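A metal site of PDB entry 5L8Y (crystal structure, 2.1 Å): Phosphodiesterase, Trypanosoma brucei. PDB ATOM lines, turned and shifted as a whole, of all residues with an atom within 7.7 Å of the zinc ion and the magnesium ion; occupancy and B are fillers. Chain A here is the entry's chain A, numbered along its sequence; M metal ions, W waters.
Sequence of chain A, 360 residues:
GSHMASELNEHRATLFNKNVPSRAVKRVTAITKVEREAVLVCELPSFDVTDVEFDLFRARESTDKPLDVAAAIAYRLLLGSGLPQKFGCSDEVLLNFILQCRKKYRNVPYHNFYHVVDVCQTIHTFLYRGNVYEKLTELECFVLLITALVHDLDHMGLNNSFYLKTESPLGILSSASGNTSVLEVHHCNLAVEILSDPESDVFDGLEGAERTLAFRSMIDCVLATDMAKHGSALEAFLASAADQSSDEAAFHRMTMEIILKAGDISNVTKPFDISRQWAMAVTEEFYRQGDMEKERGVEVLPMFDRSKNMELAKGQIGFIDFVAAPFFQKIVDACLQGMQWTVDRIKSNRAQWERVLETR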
ATOM      1  N   TYR A 105     -26.694  11.962 -23.965  1.00  0.00           N
ATOM      2  CA  TYR A 105     -27.655  10.928 -24.363  1.00  0.00           C
ATOM      3  C   TYR A 105     -28.433  11.432 -25.542  1.00  0.00           C
ATOM      4  O   TYR A 105     -28.614  12.637 -25.711  1.00  0.00           O
ATOM      5  CB  TYR A 105     -28.603  10.509 -23.214  1.00  0.00           C
ATOM      6  CG  TYR A 105     -27.839   9.681 -22.225  1.00  0.00           C
ATOM      7  CD1 TYR A 105     -27.669   8.316 -22.426  1.00  0.00           C
ATOM      8  CD2 TYR A 105     -27.186  10.277 -21.160  1.00  0.00           C
ATOM      9  CE1 TYR A 105     -26.908   7.565 -21.558  1.00  0.00           C
ATOM     10  CE2 TYR A 105     -26.442   9.533 -20.269  1.00  0.00           C
ATOM     11  CZ  TYR A 105     -26.308   8.165 -20.480  1.00  0.00           C
ATOM     12  OH  TYR A 105     -25.562   7.429 -19.639  1.00  0.00           O
ATOM     13  N   TYR A 110     -34.980   3.624 -26.393  1.00  0.00           N
ATOM     14  CA  TYR A 110     -34.698   2.987 -25.087  1.00  0.00           C
ATOM     15  C   TYR A 110     -33.444   3.490 -24.399  1.00  0.00           C
ATOM     16  O   TYR A 110     -33.510   3.936 -23.275  1.00  0.00           O
ATOM     17  CB  TYR A 110     -34.636   1.462 -25.228  1.00  0.00           C
ATOM     18  CG  TYR A 110     -34.407   0.737 -23.907  1.00  0.00           C
ATOM     19  CD1 TYR A 110     -35.415   0.676 -22.933  1.00  0.00           C
ATOM     20  CD2 TYR A 110     -33.196   0.088 -23.632  1.00  0.00           C
ATOM     21  CE1 TYR A 110     -35.236   0.001 -21.733  1.00  0.00           C
ATOM     22  CE2 TYR A 110     -32.998  -0.582 -22.421  1.00  0.00           C
ATOM     23  CZ  TYR A 110     -34.029  -0.635 -21.476  1.00  0.00           C
ATOM     24  OH  TYR A 110     -33.882  -1.290 -20.277  1.00  0.00           O
ATOM     25  N   HIS A 111     -32.291   3.464 -25.070  1.00  0.00           N
ATOM     26  CA  HIS A 111     -31.037   3.879 -24.432  1.00  0.00           C
ATOM     27  C   HIS A 111     -30.838   5.392 -24.422  1.00  0.00           C
ATOM     28  O   HIS A 111     -29.859   5.909 -24.951  1.00  0.00           O
ATOM     29  CB  HIS A 111     -29.838   3.187 -25.074  1.00  0.00           C
ATOM     30  CG  HIS A 111     -29.830   1.729 -24.827  1.00  0.00           C
ATOM     31  ND1 HIS A 111     -30.208   0.814 -25.770  1.00  0.00           N
ATOM     32  CD2 HIS A 111     -29.511   1.020 -23.722  1.00  0.00           C
ATOM     33  CE1 HIS A 111     -30.092  -0.410 -25.271  1.00  0.00           C
ATOM     34  NE2 HIS A 111     -29.682  -0.308 -24.022  1.00  0.00           N
ATOM     35  N   ASN A 112     -31.770   6.063 -23.771  1.00  0.00           N
ATOM     36  CA  ASN A 112     -31.785   7.501 -23.660  1.00  0.00           C
ATOM     37  C   ASN A 112     -31.543   7.850 -22.195  1.00  0.00           C
ATOM     38  O   ASN A 112     -31.323   6.954 -21.399  1.00  0.00           O
ATOM     39  CB  ASN A 112     -33.129   8.053 -24.181  1.00  0.00           C
ATOM     40  CG  ASN A 112     -34.343   7.414 -23.503  1.00  0.00           C
ATOM     41  OD1 ASN A 112     -34.418   7.331 -22.276  1.00  0.00           O
ATOM     42  ND2 ASN A 112     -35.280   6.947 -24.323  1.00  0.00           N
ATOM     43  N   HIS A 115     -33.619   5.983 -19.364  1.00  0.00           N
ATOM     44  CA  HIS A 115     -33.089   4.712 -18.985  1.00  0.00           C
ATOM     45  C   HIS A 115     -32.029   4.810 -17.883  1.00  0.00           C
ATOM     46  O   HIS A 115     -32.054   4.038 -16.926  1.00  0.00           O
ATOM     47  CB  HIS A 115     -32.527   3.987 -20.209  1.00  0.00           C
ATOM     48  CG  HIS A 115     -31.753   2.762 -19.878  1.00  0.00           C
ATOM     49  ND1 HIS A 115     -32.324   1.657 -19.287  1.00  0.00           N
ATOM     50  CD2 HIS A 115     -30.444   2.485 -20.021  1.00  0.00           C
ATOM     51  CE1 HIS A 115     -31.401   0.722 -19.122  1.00  0.00           C
ATOM     52  NE2 HIS A 115     -30.251   1.205 -19.554  1.00  0.00           N
ATOM     53  N   VAL A 116     -31.106   5.734 -17.996  1.00  0.00           N
ATOM     54  CA  VAL A 116     -30.011   5.747 -17.033  1.00  0.00           C
ATOM     55  C   VAL A 116     -30.464   6.335 -15.712  1.00  0.00           C
ATOM     56  O   VAL A 116     -29.953   5.952 -14.655  1.00  0.00           O
ATOM     57  CB  VAL A 116     -28.696   6.414 -17.579  1.00  0.00           C
ATOM     58  CG1 VAL A 116     -28.269   5.749 -18.872  1.00  0.00           C
ATOM     59  CG2 VAL A 116     -28.820   7.911 -17.765  1.00  0.00           C
ATOM     60  N   VAL A 119     -32.117   3.400 -14.150  1.00  0.00           N
ATOM     61  CA  VAL A 119     -31.121   2.484 -13.599  1.00  0.00           C
ATOM     62  C   VAL A 119     -30.553   3.029 -12.293  1.00  0.00           C
ATOM     63  O   VAL A 119     -30.465   2.319 -11.303  1.00  0.00           O
ATOM     64  CB  VAL A 119     -30.003   2.207 -14.592  1.00  0.00           C
ATOM     65  CG1 VAL A 119     -28.863   1.420 -13.919  1.00  0.00           C
ATOM     66  CG2 VAL A 119     -30.569   1.428 -15.807  1.00  0.00           C
ATOM     67  N   ALA A 148     -24.451   4.597 -12.759  1.00  0.00           N
ATOM     68  CA  ALA A 148     -25.722   4.458 -13.472  1.00  0.00           C
ATOM     69  C   ALA A 148     -25.915   5.527 -14.533  1.00  0.00           C
ATOM     70  O   ALA A 148     -26.339   5.225 -15.626  1.00  0.00           O
ATOM     71  CB  ALA A 148     -26.876   4.463 -12.489  1.00  0.00           C
ATOM     72  N   HIS A 151     -23.420   5.006 -17.746  1.00  0.00           N
ATOM     73  CA  HIS A 151     -23.137   3.664 -18.235  1.00  0.00           C
ATOM     74  C   HIS A 151     -23.574   3.371 -19.683  1.00  0.00           C
ATOM     75  O   HIS A 151     -23.126   2.391 -20.261  1.00  0.00           O
ATOM     76  CB  HIS A 151     -23.713   2.604 -17.291  1.00  0.00           C
ATOM     77  CG  HIS A 151     -25.140   2.247 -17.568  1.00  0.00           C
ATOM     78  ND1 HIS A 151     -26.188   2.960 -17.029  1.00  0.00           N
ATOM     79  CD2 HIS A 151     -25.690   1.257 -18.309  1.00  0.00           C
ATOM     80  CE1 HIS A 151     -27.327   2.432 -17.437  1.00  0.00           C
ATOM     81  NE2 HIS A 151     -27.044   1.399 -18.208  1.00  0.00           N
ATOM     82  N   ASP A 152     -24.448   4.188 -20.250  1.00  0.00           N
ATOM     83  CA  ASP A 152     -24.792   4.132 -21.690  1.00  0.00           C
ATOM     84  C   ASP A 152     -24.504   5.451 -22.490  1.00  0.00           C
ATOM     85  O   ASP A 152     -25.108   5.665 -23.536  1.00  0.00           O
ATOM     86  CB  ASP A 152     -26.270   3.774 -21.841  1.00  0.00           C
ATOM     87  CG  ASP A 152     -26.540   2.309 -21.615  1.00  0.00           C
ATOM     88  OD1 ASP A 152     -25.800   1.431 -22.103  1.00  0.00           O
ATOM     89  OD2 ASP A 152     -27.541   2.030 -20.933  1.00  0.00           O
ATOM     90  N   LEU A 153     -23.590   6.301 -22.023  1.00  0.00           N
ATOM     91  CA  LEU A 153     -23.362   7.608 -22.687  1.00  0.00           C
ATOM     92  C   LEU A 153     -23.172   7.515 -24.219  1.00  0.00           C
ATOM     93  O   LEU A 153     -22.328   6.749 -24.693  1.00  0.00           O
ATOM     94  CB  LEU A 153     -22.144   8.324 -22.130  1.00  0.00           C
ATOM     95  CG  LEU A 153     -22.251   8.872 -20.717  1.00  0.00           C
ATOM     96  CD1 LEU A 153     -20.845   9.052 -20.185  1.00  0.00           C
ATOM     97  CD2 LEU A 153     -23.042  10.163 -20.611  1.00  0.00           C
ATOM     98  N   HIS A 155     -25.176   6.341 -26.580  1.00  0.00           N
ATOM     99  CA  HIS A 155     -25.728   5.158 -27.245  1.00  0.00           C
ATOM    100  C   HIS A 155     -26.601   5.624 -28.415  1.00  0.00           C
ATOM    101  O   HIS A 155     -27.391   6.564 -28.273  1.00  0.00           O
ATOM    102  CB  HIS A 155     -26.586   4.368 -26.229  1.00  0.00           C
ATOM    103  CG  HIS A 155     -26.745   2.920 -26.538  1.00  0.00           C
ATOM    104  ND1 HIS A 155     -27.453   2.463 -27.628  1.00  0.00           N
ATOM    105  CD2 HIS A 155     -26.337   1.824 -25.870  1.00  0.00           C
ATOM    106  CE1 HIS A 155     -27.448   1.144 -27.631  1.00  0.00           C
ATOM    107  NE2 HIS A 155     -26.767   0.728 -26.576  1.00  0.00           N
ATOM    108  N   ASN A 160     -23.548  -3.748 -30.032  1.00  0.00           N
ATOM    109  CA  ASN A 160     -22.162  -4.011 -30.422  1.00  0.00           C
ATOM    110  C   ASN A 160     -22.101  -4.766 -31.722  1.00  0.00           C
ATOM    111  O   ASN A 160     -21.279  -4.464 -32.591  1.00  0.00           O
ATOM    112  CB  ASN A 160     -21.415  -4.787 -29.299  1.00  0.00           C
ATOM    113  CG  ASN A 160     -21.096  -3.914 -28.125  1.00  0.00           C
ATOM    114  OD1 ASN A 160     -20.889  -2.711 -28.283  1.00  0.00           O
ATOM    115  ND2 ASN A 160     -21.000  -4.503 -26.942  1.00  0.00           N
ATOM    116  N   LEU A 183     -19.419  -0.521 -27.462  1.00  0.00           N
ATOM    117  CA  LEU A 183     -20.179   0.539 -26.805  1.00  0.00           C
ATOM    118  C   LEU A 183     -19.643   0.831 -25.426  1.00  0.00           C
ATOM    119  O   LEU A 183     -19.498   1.993 -25.048  1.00  0.00           O
ATOM    120  CB  LEU A 183     -21.651   0.174 -26.691  1.00  0.00           C
ATOM    121  CG  LEU A 183     -22.427   0.126 -28.012  1.00  0.00           C
ATOM    122  CD1 LEU A 183     -23.696  -0.703 -27.870  1.00  0.00           C
ATOM    123  CD2 LEU A 183     -22.759   1.538 -28.459  1.00  0.00           C
ATOM    124  N   GLU A 184     -19.326  -0.223 -24.694  1.00  0.00           N
ATOM    125  CA  GLU A 184     -18.995  -0.051 -23.270  1.00  0.00           C
ATOM    126  C   GLU A 184     -17.701   0.711 -23.094  1.00  0.00           C
ATOM    127  O   GLU A 184     -17.591   1.581 -22.216  1.00  0.00           O
ATOM    128  CB  GLU A 184     -18.983  -1.371 -22.518  1.00  0.00           C
ATOM    129  CG  GLU A 184     -20.359  -2.057 -22.388  1.00  0.00           C
ATOM    130  CD  GLU A 184     -20.910  -2.691 -23.682  1.00  0.00           C
ATOM    131  OE1 GLU A 184     -20.145  -2.975 -24.649  1.00  0.00           O
ATOM    132  OE2 GLU A 184     -22.143  -2.886 -23.729  1.00  0.00           O
ATOM    133  N   HIS A 187     -18.618   4.301 -23.862  1.00  0.00           N
ATOM    134  CA  HIS A 187     -19.275   4.942 -22.701  1.00  0.00           C
ATOM    135  C   HIS A 187     -18.234   5.364 -21.702  1.00  0.00           C
ATOM    136  O   HIS A 187     -18.317   6.465 -21.150  1.00  0.00           O
ATOM    137  CB  HIS A 187     -20.314   4.050 -21.974  1.00  0.00           C
ATOM    138  CG  HIS A 187     -21.323   3.398 -22.864  1.00  0.00           C
ATOM    139  ND1 HIS A 187     -21.999   4.077 -23.853  1.00  0.00           N
ATOM    140  CD2 HIS A 187     -21.780   2.128 -22.902  1.00  0.00           C
ATOM    141  CE1 HIS A 187     -22.793   3.252 -24.492  1.00  0.00           C
ATOM    142  NE2 HIS A 187     -22.703   2.067 -23.911  1.00  0.00           N
ATOM    143  N   VAL A 222     -19.121  -0.561 -15.853  1.00  0.00           N
ATOM    144  CA  VAL A 222     -19.630  -0.270 -17.190  1.00  0.00           C
ATOM    145  C   VAL A 222     -19.250  -1.393 -18.142  1.00  0.00           C
ATOM    146  O   VAL A 222     -20.084  -1.823 -18.917  1.00  0.00           O
ATOM    147  CB  VAL A 222     -19.098   1.081 -17.739  1.00  0.00           C
ATOM    148  CG1 VAL A 222     -19.567   1.312 -19.181  1.00  0.00           C
ATOM    149  CG2 VAL A 222     -19.512   2.218 -16.838  1.00  0.00           C
ATOM    150  N   THR A 225     -21.433  -4.494 -18.076  1.00  0.00           N
ATOM    151  CA  THR A 225     -22.824  -4.419 -18.583  1.00  0.00           C
ATOM    152  C   THR A 225     -22.967  -4.983 -19.996  1.00  0.00           C
ATOM    153  O   THR A 225     -24.095  -5.097 -20.499  1.00  0.00           O
ATOM    154  CB  THR A 225     -23.416  -2.978 -18.533  1.00  0.00           C
ATOM    155  OG1 THR A 225     -22.696  -2.063 -19.380  1.00  0.00           O
ATOM    156  CG2 THR A 225     -23.397  -2.448 -17.119  1.00  0.00           C
ATOM    157  N   ASP A 226     -21.854  -5.303 -20.649  1.00  0.00           N
ATOM    158  CA  ASP A 226     -21.892  -5.938 -21.962  1.00  0.00           C
ATOM    159  C   ASP A 226     -22.489  -7.330 -21.776  1.00  0.00           C
ATOM    160  O   ASP A 226     -21.926  -8.151 -21.057  1.00  0.00           O
ATOM    161  CB  ASP A 226     -20.475  -6.064 -22.518  1.00  0.00           C
ATOM    162  CG  ASP A 226     -20.420  -6.789 -23.867  1.00  0.00           C
ATOM    163  OD1 ASP A 226     -21.402  -7.417 -24.304  1.00  0.00           O
ATOM    164  OD2 ASP A 226     -19.367  -6.726 -24.517  1.00  0.00           O
ATOM    165  N   MET A 227     -23.648  -7.593 -22.393  1.00  0.00           N
ATOM    166  CA  MET A 227     -24.398  -8.843 -22.138  1.00  0.00           C
ATOM    167  C   MET A 227     -23.721 -10.092 -22.700  1.00  0.00           C
ATOM    168  O   MET A 227     -24.066 -11.209 -22.289  1.00  0.00           O
ATOM    169  CB  MET A 227     -25.868  -8.750 -22.628  1.00  0.00           C
ATOM    170  CG  MET A 227     -26.786  -7.961 -21.693  1.00  0.00           C
ATOM    171  SD  MET A 227     -26.892  -8.586 -19.982  1.00  0.00           S
ATOM    172  CE  MET A 227     -27.833 -10.091 -20.237  1.00  0.00           C
ATOM    173  N   LEU A 260     -25.005  -3.136 -10.826  1.00  0.00           N
ATOM    174  CA  LEU A 260     -25.226  -2.345 -12.037  1.00  0.00           C
ATOM    175  C   LEU A 260     -25.861  -3.183 -13.097  1.00  0.00           C
ATOM    176  O   LEU A 260     -26.806  -2.718 -13.724  1.00  0.00           O
ATOM    177  CB  LEU A 260     -23.958  -1.675 -12.577  1.00  0.00           C
ATOM    178  CG  LEU A 260     -24.153  -0.867 -13.886  1.00  0.00           C
ATOM    179  CD1 LEU A 260     -25.076   0.321 -13.715  1.00  0.00           C
ATOM    180  CD2 LEU A 260     -22.825  -0.376 -14.425  1.00  0.00           C
ATOM    181  N   GLY A 263     -29.588  -3.565 -12.191  1.00  0.00           N
ATOM    182  CA  GLY A 263     -30.304  -2.371 -12.598  1.00  0.00           C
ATOM    183  C   GLY A 263     -30.607  -2.309 -14.080  1.00  0.00           C
ATOM    184  O   GLY A 263     -31.695  -1.924 -14.497  1.00  0.00           O
ATOM    185  N   ASP A 264     -29.629  -2.711 -14.873  1.00  0.00           N
ATOM    186  CA  ASP A 264     -29.753  -2.729 -16.314  1.00  0.00           C
ATOM    187  C   ASP A 264     -30.801  -3.685 -16.839  1.00  0.00           C
ATOM    188  O   ASP A 264     -31.387  -3.383 -17.849  1.00  0.00           O
ATOM    189  CB  ASP A 264     -28.418  -3.145 -16.966  1.00  0.00           C
ATOM    190  CG  ASP A 264     -28.113  -2.375 -18.218  1.00  0.00           C
ATOM    191  OD1 ASP A 264     -28.705  -1.306 -18.423  1.00  0.00           O
ATOM    192  OD2 ASP A 264     -27.170  -2.779 -18.924  1.00  0.00           O
ATOM    193  N   ILE A 265     -30.994  -4.849 -16.192  1.00  0.00           N
ATOM    194  CA  ILE A 265     -32.065  -5.780 -16.580  1.00  0.00           C
ATOM    195  C   ILE A 265     -33.249  -5.805 -15.596  1.00  0.00           C
ATOM    196  O   ILE A 265     -33.912  -6.818 -15.448  1.00  0.00           O
ATOM    197  CB  ILE A 265     -31.553  -7.197 -16.824  1.00  0.00           C
ATOM    198  CG1 ILE A 265     -30.849  -7.747 -15.607  1.00  0.00           C
ATOM    199  CG2 ILE A 265     -30.604  -7.221 -18.011  1.00  0.00           C
ATOM    200  CD1 ILE A 265     -30.614  -9.234 -15.706  1.00  0.00           C
HETATM  201 ZN    ZN M   1     -28.188   0.367 -19.783  1.00  0.00          ZN
HETATM  202 MG    MG M   2     -25.161  -0.486 -22.162  1.00  0.00          MG
HETATM  203  O   HOH W   1     -23.305  -0.320 -21.071  1.00  0.00           O
HETATM  204  O   HOH W   2     -29.103  -1.143 -21.433  1.00  0.00           O
HETATM  205  O   HOH W   3     -24.513  -2.539 -22.191  1.00  0.00           O
HETATM  206  O   HOH W   4     -26.627  -0.734 -20.836  1.00  0.00           O
HETATM  207  O   HOH W   5     -26.912  -0.727 -23.618  1.00  0.00           O
HETATM  208  O   HOH W   6     -24.137  -0.333 -23.975  1.00  0.00           O
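N of Asp 152 is in hydrogen-bond range of OH of Tyr 105. O of Ala 148 lies within hydrogen-bond range of ND1 of His 151 (2.7 Å). OH of Tyr 110 lies close to ND1 of His 115, at 3.5 Å. N of His 115 sits at hydrogen-bond distance from OD1 of Asn 112 (3.3 Å). O of Leu 183 sits close to NE2 of His 187, at 3.4 Å. ND1 of His 187 is in hydrogen-bond range of O of Leu 153, at 2.8 Å.
Of the 24 residues printed, 4 come within 4 Å of the zinc ion.
Merely in contact with the magnesium ion: His 187.
OD2 of Asp 152 is bound to the zinc ion. The zinc ion is bound by water W4, 2.2 Å away. NE2 of His 151 is bound to the zinc ion (2.2 Å). The zinc ion is bound by OD1 of Asp 264 (2.2 Å). The zinc ion is bound by NE2 of His 115, 2.2 Å away. The zinc ion is bound by water W2 (2.4 Å). The zinc ion has six donor atoms within binding distance.
Water W4 binds the magnesium ion, 2.0 Å away. OD1 of Asp 152 is bound to the magnesium ion, 2.0 Å away. Water W6 binds the magnesium ion (2.1 Å). Water W3 is bound to the magnesium ion, 2.2 Å away. Water W1 is bound to the magnesium ion. Water W5 is bound to the magnesium ion, at 2.3 Å. The magnesium ion has six donor atoms within binding distance.
Water W1 bridges the side-chain hydroxyl (OG1) of Thr 225 and the backbone carbonyl oxygen (O) of His 151. Water W6 bridges a ring nitrogen (NE2) of His 187 (2.8 Å) and the side-chain carboxylate of Glu 184 (3.2 Å). Water W3 lies within hydrogen-bond range of the side-chain carboxylate of Glu 184 (2.8 Å) and the backbone carbonyl oxygen of Thr 225 (3.1 Å). Water W5 bridges a ring nitrogen (NE2) of His 111 (2.8 Å) and a ring nitrogen (NE2) of His 155 (3.3 Å).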
